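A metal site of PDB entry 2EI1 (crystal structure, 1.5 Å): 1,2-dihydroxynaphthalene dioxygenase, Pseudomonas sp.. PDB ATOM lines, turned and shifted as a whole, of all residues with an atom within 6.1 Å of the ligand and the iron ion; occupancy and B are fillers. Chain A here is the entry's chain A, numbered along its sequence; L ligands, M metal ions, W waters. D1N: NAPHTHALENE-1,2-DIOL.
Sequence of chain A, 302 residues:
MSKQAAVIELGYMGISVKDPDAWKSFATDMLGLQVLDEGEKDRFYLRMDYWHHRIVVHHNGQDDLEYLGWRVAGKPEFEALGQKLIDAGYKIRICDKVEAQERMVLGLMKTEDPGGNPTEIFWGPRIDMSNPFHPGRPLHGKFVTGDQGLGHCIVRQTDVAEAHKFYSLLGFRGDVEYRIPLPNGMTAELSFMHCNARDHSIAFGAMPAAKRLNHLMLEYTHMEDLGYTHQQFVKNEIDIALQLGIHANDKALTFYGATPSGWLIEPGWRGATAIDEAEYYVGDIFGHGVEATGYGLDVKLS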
ATOM      1  N   HIS A 152       2.450   9.855 -13.212  1.00  0.00           N
ATOM      2  CA  HIS A 152       1.530  10.447 -12.257  1.00  0.00           C
ATOM      3  C   HIS A 152       1.977  11.827 -11.838  1.00  0.00           C
ATOM      4  O   HIS A 152       3.121  12.221 -12.075  1.00  0.00           O
ATOM      5  CB  HIS A 152       1.323   9.549 -11.015  1.00  0.00           C
ATOM      6  CG  HIS A 152       2.477   9.514 -10.058  1.00  0.00           C
ATOM      7  ND1 HIS A 152       3.160   8.340  -9.788  1.00  0.00           N
ATOM      8  CD2 HIS A 152       3.019  10.451  -9.245  1.00  0.00           C
ATOM      9  CE1 HIS A 152       4.075   8.571  -8.859  1.00  0.00           C
ATOM     10  NE2 HIS A 152       4.012   9.848  -8.519  1.00  0.00           N
ATOM     11  N   CYS A 153       1.070  12.571 -11.202  1.00  0.00           N
ATOM     12  CA  CYS A 153       1.455  13.849 -10.595  1.00  0.00           C
ATOM     13  C   CYS A 153       0.802  14.061  -9.240  1.00  0.00           C
ATOM     14  O   CYS A 153      -0.276  13.527  -8.982  1.00  0.00           O
ATOM     15  CB  CYS A 153       1.056  15.064 -11.426  1.00  0.00           C
ATOM     16  SG  CYS A 153       1.428  15.198 -13.166  1.00  0.00           S
ATOM     17  N   ILE A 154       1.449  14.893  -8.417  1.00  0.00           N
ATOM     18  CA  ILE A 154       0.752  15.563  -7.313  1.00  0.00           C
ATOM     19  C   ILE A 154       0.440  16.963  -7.812  1.00  0.00           C
ATOM     20  O   ILE A 154       1.325  17.654  -8.329  1.00  0.00           O
ATOM     21  CB  ILE A 154       1.569  15.614  -6.000  1.00  0.00           C
ATOM     22  CG1 ILE A 154       1.595  14.215  -5.340  1.00  0.00           C
ATOM     23  CG2 ILE A 154       1.003  16.676  -5.026  1.00  0.00           C
ATOM     24  CD1 ILE A 154       2.269  14.194  -3.964  1.00  0.00           C
ATOM     25  N   TYR A 178      -1.098   8.071   3.241  1.00  0.00           N
ATOM     26  CA  TYR A 178      -0.040   8.418   4.181  1.00  0.00           C
ATOM     27  C   TYR A 178      -0.515   9.370   5.246  1.00  0.00           C
ATOM     28  O   TYR A 178      -1.181  10.351   4.930  1.00  0.00           O
ATOM     29  CB  TYR A 178       1.135   9.083   3.478  1.00  0.00           C
ATOM     30  CG  TYR A 178       1.998   8.120   2.702  1.00  0.00           C
ATOM     31  CD1 TYR A 178       1.558   7.614   1.485  1.00  0.00           C
ATOM     32  CD2 TYR A 178       3.252   7.740   3.156  1.00  0.00           C
ATOM     33  CE1 TYR A 178       2.338   6.747   0.727  1.00  0.00           C
ATOM     34  CE2 TYR A 178       4.061   6.862   2.404  1.00  0.00           C
ATOM     35  CZ  TYR A 178       3.582   6.366   1.196  1.00  0.00           C
ATOM     36  OH  TYR A 178       4.333   5.524   0.385  1.00  0.00           O
ATOM     37  N   ILE A 180       1.679  11.240   7.799  1.00  0.00           N
ATOM     38  CA  ILE A 180       3.085  11.535   8.088  1.00  0.00           C
ATOM     39  C   ILE A 180       3.164  12.540   9.245  1.00  0.00           C
ATOM     40  O   ILE A 180       2.623  13.636   9.140  1.00  0.00           O
ATOM     41  CB  ILE A 180       3.785  12.174   6.862  1.00  0.00           C
ATOM     42  CG1 ILE A 180       3.711  11.238   5.651  1.00  0.00           C
ATOM     43  CG2 ILE A 180       5.234  12.558   7.210  1.00  0.00           C
ATOM     44  CD1 ILE A 180       3.749  11.972   4.311  1.00  0.00           C
ATOM     45  N   LEU A 190      -1.944  12.465   2.841  1.00  0.00           N
ATOM     46  CA  LEU A 190      -1.864  12.534   1.379  1.00  0.00           C
ATOM     47  C   LEU A 190      -2.732  11.435   0.797  1.00  0.00           C
ATOM     48  O   LEU A 190      -2.691  10.306   1.275  1.00  0.00           O
ATOM     49  CB  LEU A 190      -0.415  12.384   0.897  1.00  0.00           C
ATOM     50  CG  LEU A 190       0.498  13.587   1.164  1.00  0.00           C
ATOM     51  CD1 LEU A 190       1.915  13.254   0.745  1.00  0.00           C
ATOM     52  CD2 LEU A 190       0.017  14.800   0.401  1.00  0.00           C
ATOM     53  N   PHE A 192      -4.116   9.302  -2.699  1.00  0.00           N
ATOM     54  CA  PHE A 192      -3.562   8.793  -3.970  1.00  0.00           C
ATOM     55  C   PHE A 192      -4.645   8.040  -4.698  1.00  0.00           C
ATOM     56  O   PHE A 192      -5.247   7.113  -4.120  1.00  0.00           O
ATOM     57  CB  PHE A 192      -2.382   7.830  -3.714  1.00  0.00           C
ATOM     58  CG  PHE A 192      -1.221   8.483  -3.024  1.00  0.00           C
ATOM     59  CD1 PHE A 192      -1.271   8.775  -1.654  1.00  0.00           C
ATOM     60  CD2 PHE A 192      -0.056   8.806  -3.733  1.00  0.00           C
ATOM     61  CE1 PHE A 192      -0.205   9.387  -1.000  1.00  0.00           C
ATOM     62  CE2 PHE A 192       1.009   9.440  -3.085  1.00  0.00           C
ATOM     63  CZ  PHE A 192       0.944   9.731  -1.732  1.00  0.00           C
ATOM     64  N   ASP A 199       0.073   2.366  -9.930  1.00  0.00           N
ATOM     65  CA  ASP A 199      -0.338   2.463  -8.526  1.00  0.00           C
ATOM     66  C   ASP A 199      -1.171   3.704  -8.252  1.00  0.00           C
ATOM     67  O   ASP A 199      -2.189   3.639  -7.553  1.00  0.00           O
ATOM     68  CB  ASP A 199       0.838   2.427  -7.575  1.00  0.00           C
ATOM     69  CG  ASP A 199       0.405   2.650  -6.148  1.00  0.00           C
ATOM     70  OD1 ASP A 199      -0.047   1.653  -5.541  1.00  0.00           O
ATOM     71  OD2 ASP A 199       0.466   3.808  -5.702  1.00  0.00           O
ATOM     72  N   HIS A 200      -0.762   4.841  -8.801  1.00  0.00           N
ATOM     73  CA  HIS A 200      -1.645   6.015  -8.795  1.00  0.00           C
ATOM     74  C   HIS A 200      -1.318   6.889  -9.990  1.00  0.00           C
ATOM     75  O   HIS A 200      -0.220   6.809 -10.552  1.00  0.00           O
ATOM     76  CB  HIS A 200      -1.597   6.790  -7.487  1.00  0.00           C
ATOM     77  CG  HIS A 200      -0.266   7.391  -7.178  1.00  0.00           C
ATOM     78  ND1 HIS A 200       0.782   6.653  -6.678  1.00  0.00           N
ATOM     79  CD2 HIS A 200       0.163   8.679  -7.268  1.00  0.00           C
ATOM     80  CE1 HIS A 200       1.825   7.459  -6.506  1.00  0.00           C
ATOM     81  NE2 HIS A 200       1.467   8.685  -6.854  1.00  0.00           N
ATOM     82  N   ASN A 214       3.177  19.944  -8.233  1.00  0.00           N
ATOM     83  CA  ASN A 214       4.225  19.619  -7.268  1.00  0.00           C
ATOM     84  C   ASN A 214       5.311  18.763  -7.914  1.00  0.00           C
ATOM     85  O   ASN A 214       6.493  19.114  -7.878  1.00  0.00           O
ATOM     86  CB  ASN A 214       3.667  18.903  -6.040  1.00  0.00           C
ATOM     87  CG  ASN A 214       4.768  18.431  -5.113  1.00  0.00           C
ATOM     88  OD1 ASN A 214       5.154  17.247  -5.131  1.00  0.00           O
ATOM     89  ND2 ASN A 214       5.316  19.360  -4.311  1.00  0.00           N
ATOM     90  N   HIS A 215       4.915  17.632  -8.496  1.00  0.00           N
ATOM     91  CA  HIS A 215       5.866  16.829  -9.247  1.00  0.00           C
ATOM     92  C   HIS A 215       5.172  15.988 -10.280  1.00  0.00           C
ATOM     93  O   HIS A 215       3.973  15.712 -10.160  1.00  0.00           O
ATOM     94  CB  HIS A 215       6.729  15.930  -8.331  1.00  0.00           C
ATOM     95  CG  HIS A 215       6.024  14.743  -7.755  1.00  0.00           C
ATOM     96  ND1 HIS A 215       5.270  14.820  -6.603  1.00  0.00           N
ATOM     97  CD2 HIS A 215       5.975  13.439  -8.141  1.00  0.00           C
ATOM     98  CE1 HIS A 215       4.784  13.630  -6.318  1.00  0.00           C
ATOM     99  NE2 HIS A 215       5.210  12.759  -7.219  1.00  0.00           N
ATOM    100  N   MET A 217       5.947  12.199 -12.081  1.00  0.00           N
ATOM    101  CA  MET A 217       6.733  10.973 -12.011  1.00  0.00           C
ATOM    102  C   MET A 217       6.734  10.304 -13.375  1.00  0.00           C
ATOM    103  O   MET A 217       5.660  10.114 -13.966  1.00  0.00           O
ATOM    104  CB  MET A 217       6.105  10.044 -10.970  1.00  0.00           C
ATOM    105  CG  MET A 217       6.924   8.808 -10.636  1.00  0.00           C
ATOM    106  SD  MET A 217       6.649   7.429 -11.777  1.00  0.00           S
ATOM    107  CE  MET A 217       7.780   6.244 -11.041  1.00  0.00           C
ATOM    108  N   LEU A 242      14.475  15.177  -2.748  1.00  0.00           N
ATOM    109  CA  LEU A 242      14.367  13.978  -1.934  1.00  0.00           C
ATOM    110  C   LEU A 242      15.253  12.913  -2.567  1.00  0.00           C
ATOM    111  O   LEU A 242      15.192  12.691  -3.784  1.00  0.00           O
ATOM    112  CB  LEU A 242      12.922  13.480  -1.827  1.00  0.00           C
ATOM    113  CG  LEU A 242      11.857  14.348  -1.159  1.00  0.00           C
ATOM    114  CD1 LEU A 242      10.493  13.686  -1.234  1.00  0.00           C
ATOM    115  CD2 LEU A 242      12.215  14.614   0.293  1.00  0.00           C
ATOM    116  N   HIS A 247       8.945   3.829  -2.098  1.00  0.00           N
ATOM    117  CA  HIS A 247       7.667   4.195  -1.534  1.00  0.00           C
ATOM    118  C   HIS A 247       6.943   2.980  -0.988  1.00  0.00           C
ATOM    119  O   HIS A 247       6.928   1.912  -1.615  1.00  0.00           O
ATOM    120  CB  HIS A 247       6.749   4.811  -2.590  1.00  0.00           C
ATOM    121  CG  HIS A 247       7.165   6.155  -3.061  1.00  0.00           C
ATOM    122  ND1 HIS A 247       7.316   7.250  -2.222  1.00  0.00           N
ATOM    123  CD2 HIS A 247       7.379   6.617  -4.319  1.00  0.00           C
ATOM    124  CE1 HIS A 247       7.634   8.306  -2.948  1.00  0.00           C
ATOM    125  NE2 HIS A 247       7.686   7.948  -4.223  1.00  0.00           N
ATOM    126  N   ALA A 248       6.273   3.177   0.149  1.00  0.00           N
ATOM    127  CA  ALA A 248       5.464   2.096   0.724  1.00  0.00           C
ATOM    128  C   ALA A 248       4.241   1.731  -0.108  1.00  0.00           C
ATOM    129  O   ALA A 248       3.856   0.559  -0.140  1.00  0.00           O
ATOM    130  CB  ALA A 248       5.059   2.458   2.146  1.00  0.00           C
ATOM    131  N   ASN A 249       3.648   2.710  -0.791  1.00  0.00           N
ATOM    132  CA  ASN A 249       2.488   2.377  -1.618  1.00  0.00           C
ATOM    133  C   ASN A 249       2.819   1.650  -2.922  1.00  0.00           C
ATOM    134  O   ASN A 249       2.372   0.514  -3.131  1.00  0.00           O
ATOM    135  CB  ASN A 249       1.518   3.573  -1.820  1.00  0.00           C
ATOM    136  CG  ASN A 249       2.166   4.810  -2.426  1.00  0.00           C
ATOM    137  OD1 ASN A 249       3.355   4.824  -2.781  1.00  0.00           O
ATOM    138  ND2 ASN A 249       1.366   5.857  -2.570  1.00  0.00           N
ATOM    139  N   ASP A 250       3.653   2.269  -3.771  1.00  0.00           N
ATOM    140  CA  ASP A 250       3.886   1.685  -5.099  1.00  0.00           C
ATOM    141  C   ASP A 250       5.158   0.842  -5.208  1.00  0.00           C
ATOM    142  O   ASP A 250       5.399   0.239  -6.241  1.00  0.00           O
ATOM    143  CB  ASP A 250       3.823   2.746  -6.201  1.00  0.00           C
ATOM    144  CG  ASP A 250       5.036   3.669  -6.233  1.00  0.00           C
ATOM    145  OD1 ASP A 250       5.943   3.561  -5.387  1.00  0.00           O
ATOM    146  OD2 ASP A 250       5.072   4.519  -7.140  1.00  0.00           O
ATOM    147  N   THR A 254      12.712   5.575  -6.480  1.00  0.00           N
ATOM    148  CA  THR A 254      12.602   6.895  -7.113  1.00  0.00           C
ATOM    149  C   THR A 254      13.451   7.938  -6.379  1.00  0.00           C
ATOM    150  O   THR A 254      13.852   7.721  -5.233  1.00  0.00           O
ATOM    151  CB  THR A 254      11.135   7.449  -7.144  1.00  0.00           C
ATOM    152  OG1 THR A 254      10.834   8.100  -5.902  1.00  0.00           O
ATOM    153  CG2 THR A 254      10.071   6.382  -7.450  1.00  0.00           C
ATOM    154  N   TYR A 256      13.686  12.646  -6.357  1.00  0.00           N
ATOM    155  CA  TYR A 256      13.020  13.852  -6.869  1.00  0.00           C
ATOM    156  C   TYR A 256      14.061  14.904  -7.147  1.00  0.00           C
ATOM    157  O   TYR A 256      14.814  15.286  -6.236  1.00  0.00           O
ATOM    158  CB  TYR A 256      12.007  14.409  -5.876  1.00  0.00           C
ATOM    159  CG  TYR A 256      10.874  13.488  -5.446  1.00  0.00           C
ATOM    160  CD1 TYR A 256      11.119  12.361  -4.660  1.00  0.00           C
ATOM    161  CD2 TYR A 256       9.549  13.787  -5.780  1.00  0.00           C
ATOM    162  CE1 TYR A 256      10.074  11.541  -4.232  1.00  0.00           C
ATOM    163  CE2 TYR A 256       8.512  12.984  -5.359  1.00  0.00           C
ATOM    164  CZ  TYR A 256       8.773  11.869  -4.582  1.00  0.00           C
ATOM    165  OH  TYR A 256       7.718  11.076  -4.158  1.00  0.00           O
ATOM    166  N   GLU A 266      10.106  13.258 -10.738  1.00  0.00           N
ATOM    167  CA  GLU A 266      10.371  12.075  -9.921  1.00  0.00           C
ATOM    168  C   GLU A 266      10.683  10.915 -10.877  1.00  0.00           C
ATOM    169  O   GLU A 266       9.786  10.163 -11.259  1.00  0.00           O
ATOM    170  CB  GLU A 266       9.141  11.735  -9.047  1.00  0.00           C
ATOM    171  CG  GLU A 266       9.388  10.551  -8.115  1.00  0.00           C
ATOM    172  CD  GLU A 266       8.152  10.103  -7.359  1.00  0.00           C
ATOM    173  OE1 GLU A 266       7.037  10.576  -7.665  1.00  0.00           O
ATOM    174  OE2 GLU A 266       8.313   9.221  -6.479  1.00  0.00           O
ATOM    175  N   ASP A 284       7.988   5.735   4.473  1.00  0.00           N
ATOM    176  CA  ASP A 284       8.424   4.924   3.335  1.00  0.00           C
ATOM    177  C   ASP A 284       9.302   3.735   3.757  1.00  0.00           C
ATOM    178  O   ASP A 284       9.637   3.576   4.938  1.00  0.00           O
ATOM    179  CB  ASP A 284       9.067   5.823   2.266  1.00  0.00           C
ATOM    180  CG  ASP A 284       8.056   6.284   1.218  1.00  0.00           C
ATOM    181  OD1 ASP A 284       6.910   5.759   1.201  1.00  0.00           O
ATOM    182  OD2 ASP A 284       8.395   7.151   0.378  1.00  0.00           O
ATOM    183  N   LEU A 297       7.971  19.602  -0.716  1.00  0.00           N
ATOM    184  CA  LEU A 297       7.942  18.228  -0.221  1.00  0.00           C
ATOM    185  C   LEU A 297       8.904  18.031   0.948  1.00  0.00           C
ATOM    186  O   LEU A 297       9.768  17.173   0.910  1.00  0.00           O
ATOM    187  CB  LEU A 297       8.293  17.252  -1.340  1.00  0.00           C
ATOM    188  CG  LEU A 297       7.177  16.766  -2.255  1.00  0.00           C
ATOM    189  CD1 LEU A 297       7.702  15.675  -3.175  1.00  0.00           C
ATOM    190  CD2 LEU A 297       5.987  16.251  -1.493  1.00  0.00           C
ATOM    191  N   VAL A 299       8.600  16.573   3.758  1.00  0.00           N
ATOM    192  CA  VAL A 299       7.962  15.603   4.640  1.00  0.00           C
ATOM    193  C   VAL A 299       9.010  14.624   5.156  1.00  0.00           C
ATOM    194  O   VAL A 299      10.029  14.398   4.499  1.00  0.00           O
ATOM    195  CB  VAL A 299       6.886  14.781   3.898  1.00  0.00           C
ATOM    196  CG1 VAL A 299       5.619  15.586   3.702  1.00  0.00           C
ATOM    197  CG2 VAL A 299       7.404  14.281   2.580  1.00  0.00           C
ATOM    198  N   LEU A 301       9.909  10.975   5.639  1.00  0.00           N
ATOM    199  CA  LEU A 301       9.468   9.715   5.064  1.00  0.00           C
ATOM    200  C   LEU A 301      10.331   8.575   5.584  1.00  0.00           C
ATOM    201  O   LEU A 301      10.014   7.423   5.396  1.00  0.00           O
ATOM    202  CB  LEU A 301       9.574   9.800   3.557  1.00  0.00           C
ATOM    203  CG  LEU A 301       8.355   9.936   2.655  1.00  0.00           C
ATOM    204  CD1 LEU A 301       7.001   9.853   3.306  1.00  0.00           C
ATOM    205  CD2 LEU A 301       8.449  10.966   1.569  1.00  0.00           C
HETATM  206  O2  D1N L   1       4.779   8.733  -5.866  1.00  0.00           O
HETATM  207  C2  D1N L   1       4.646   8.902  -4.458  1.00  0.00           C
HETATM  208  C3  D1N L   1       4.296   7.841  -3.612  1.00  0.00           C
HETATM  209  C4  D1N L   1       4.211   8.090  -2.242  1.00  0.00           C
HETATM  210  C5  D1N L   1       4.442   9.378  -1.721  1.00  0.00           C
HETATM  211  C10 D1N L   1       4.773  10.430  -2.580  1.00  0.00           C
HETATM  212  C1  D1N L   1       4.878  10.175  -3.944  1.00  0.00           C
HETATM  213  O1  D1N L   1       5.236  11.190  -4.887  1.00  0.00           O
HETATM  214  C9  D1N L   1       5.031  11.732  -2.082  1.00  0.00           C
HETATM  215  C8  D1N L   1       4.924  11.936  -0.702  1.00  0.00           C
HETATM  216  C7  D1N L   1       4.576  10.878   0.152  1.00  0.00           C
HETATM  217  C6  D1N L   1       4.347   9.608  -0.352  1.00  0.00           C
HETATM  218 FE    FE M   1       5.120  10.627  -6.821  1.00  0.00          FE
HETATM  219  O   HOH W   1       2.786  11.053  -6.136  1.00  0.00           O
HETATM  220  O   HOH W   2       6.413   6.846  -7.402  1.00  0.00           O
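The side-chain hydroxyl (OH) of Tyr 256 lies close to an oxygen (O1) of the ligand, 2.6 Å away.
A ring nitrogen (NE2) of His 247 lies close to an oxygen (O2) of the ligand (3.4 Å).
NE2 of His 200 sits close to O2 of the ligand (3.5 Å).
Residues that only touch the iron ion: Tyr 256 (3.7 Å).
Within 4 Å of the iron ion: His 152, His 215, Tyr 256 and Glu 266.
The nearest printed residue that does not touch the iron ion is His 200 (4.1 Å).
The iron ion is bound by an oxygen (O1) of the ligand (2.0 Å), the side-chain carboxylate of Glu 266 (2.1 Å), an oxygen (O2) of the ligand (2.1 Å), a ring nitrogen (NE2) of His 215 (2.2 Å), a ring nitrogen (NE2) of His 152 (2.2 Å) and water W1 (2.5 Å).
The side-chain carboxylate (OE2) of Glu 266 lies within hydrogen-bond range of the side-chain hydroxyl (OH) of Tyr 256.
OE2 of Glu 266 lies within hydrogen-bond range of NE2 of His 247 (2.7 Å).
The backbone carbonyl oxygen (O) of His 215 sits at hydrogen-bond distance from the backbone NH (N) of Ile 154 (3.2 Å).
A ring nitrogen (ND1) of His 215 lies within hydrogen-bond range of the side-chain amide oxygen (OD1) of Asn 214.
ND1 of His 152 sits close to NE2 of His 200, at 3.4 Å.
The side-chain hydroxyl of Tyr 256 sits close to a ring nitrogen (NE2) of His 247 (3.1 Å).
The backbone NH (N) of Tyr 256 lies within hydrogen-bond range of the backbone carbonyl oxygen (O) of Leu 242, at 3.0 Å.
ND1 of His 247 lies within hydrogen-bond range of OD2 of Asp 284, 2.8 Å away.
Merely in contact with the ligand: Asn 249 (3.3 Å), Phe 192 (3.5 Å), Leu 190 (3.6 Å) and Tyr 178 (3.7 Å).
Ten residues have an atom within 4 Å of the ligand: His 152, Tyr 178, Leu 190, Phe 192, His 200, His 215, His 247, Asn 249, Tyr 256 and Glu 266.
Water W2 lies within hydrogen-bond range of OD2 of Asp 250 and OE2 of Glu 266.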
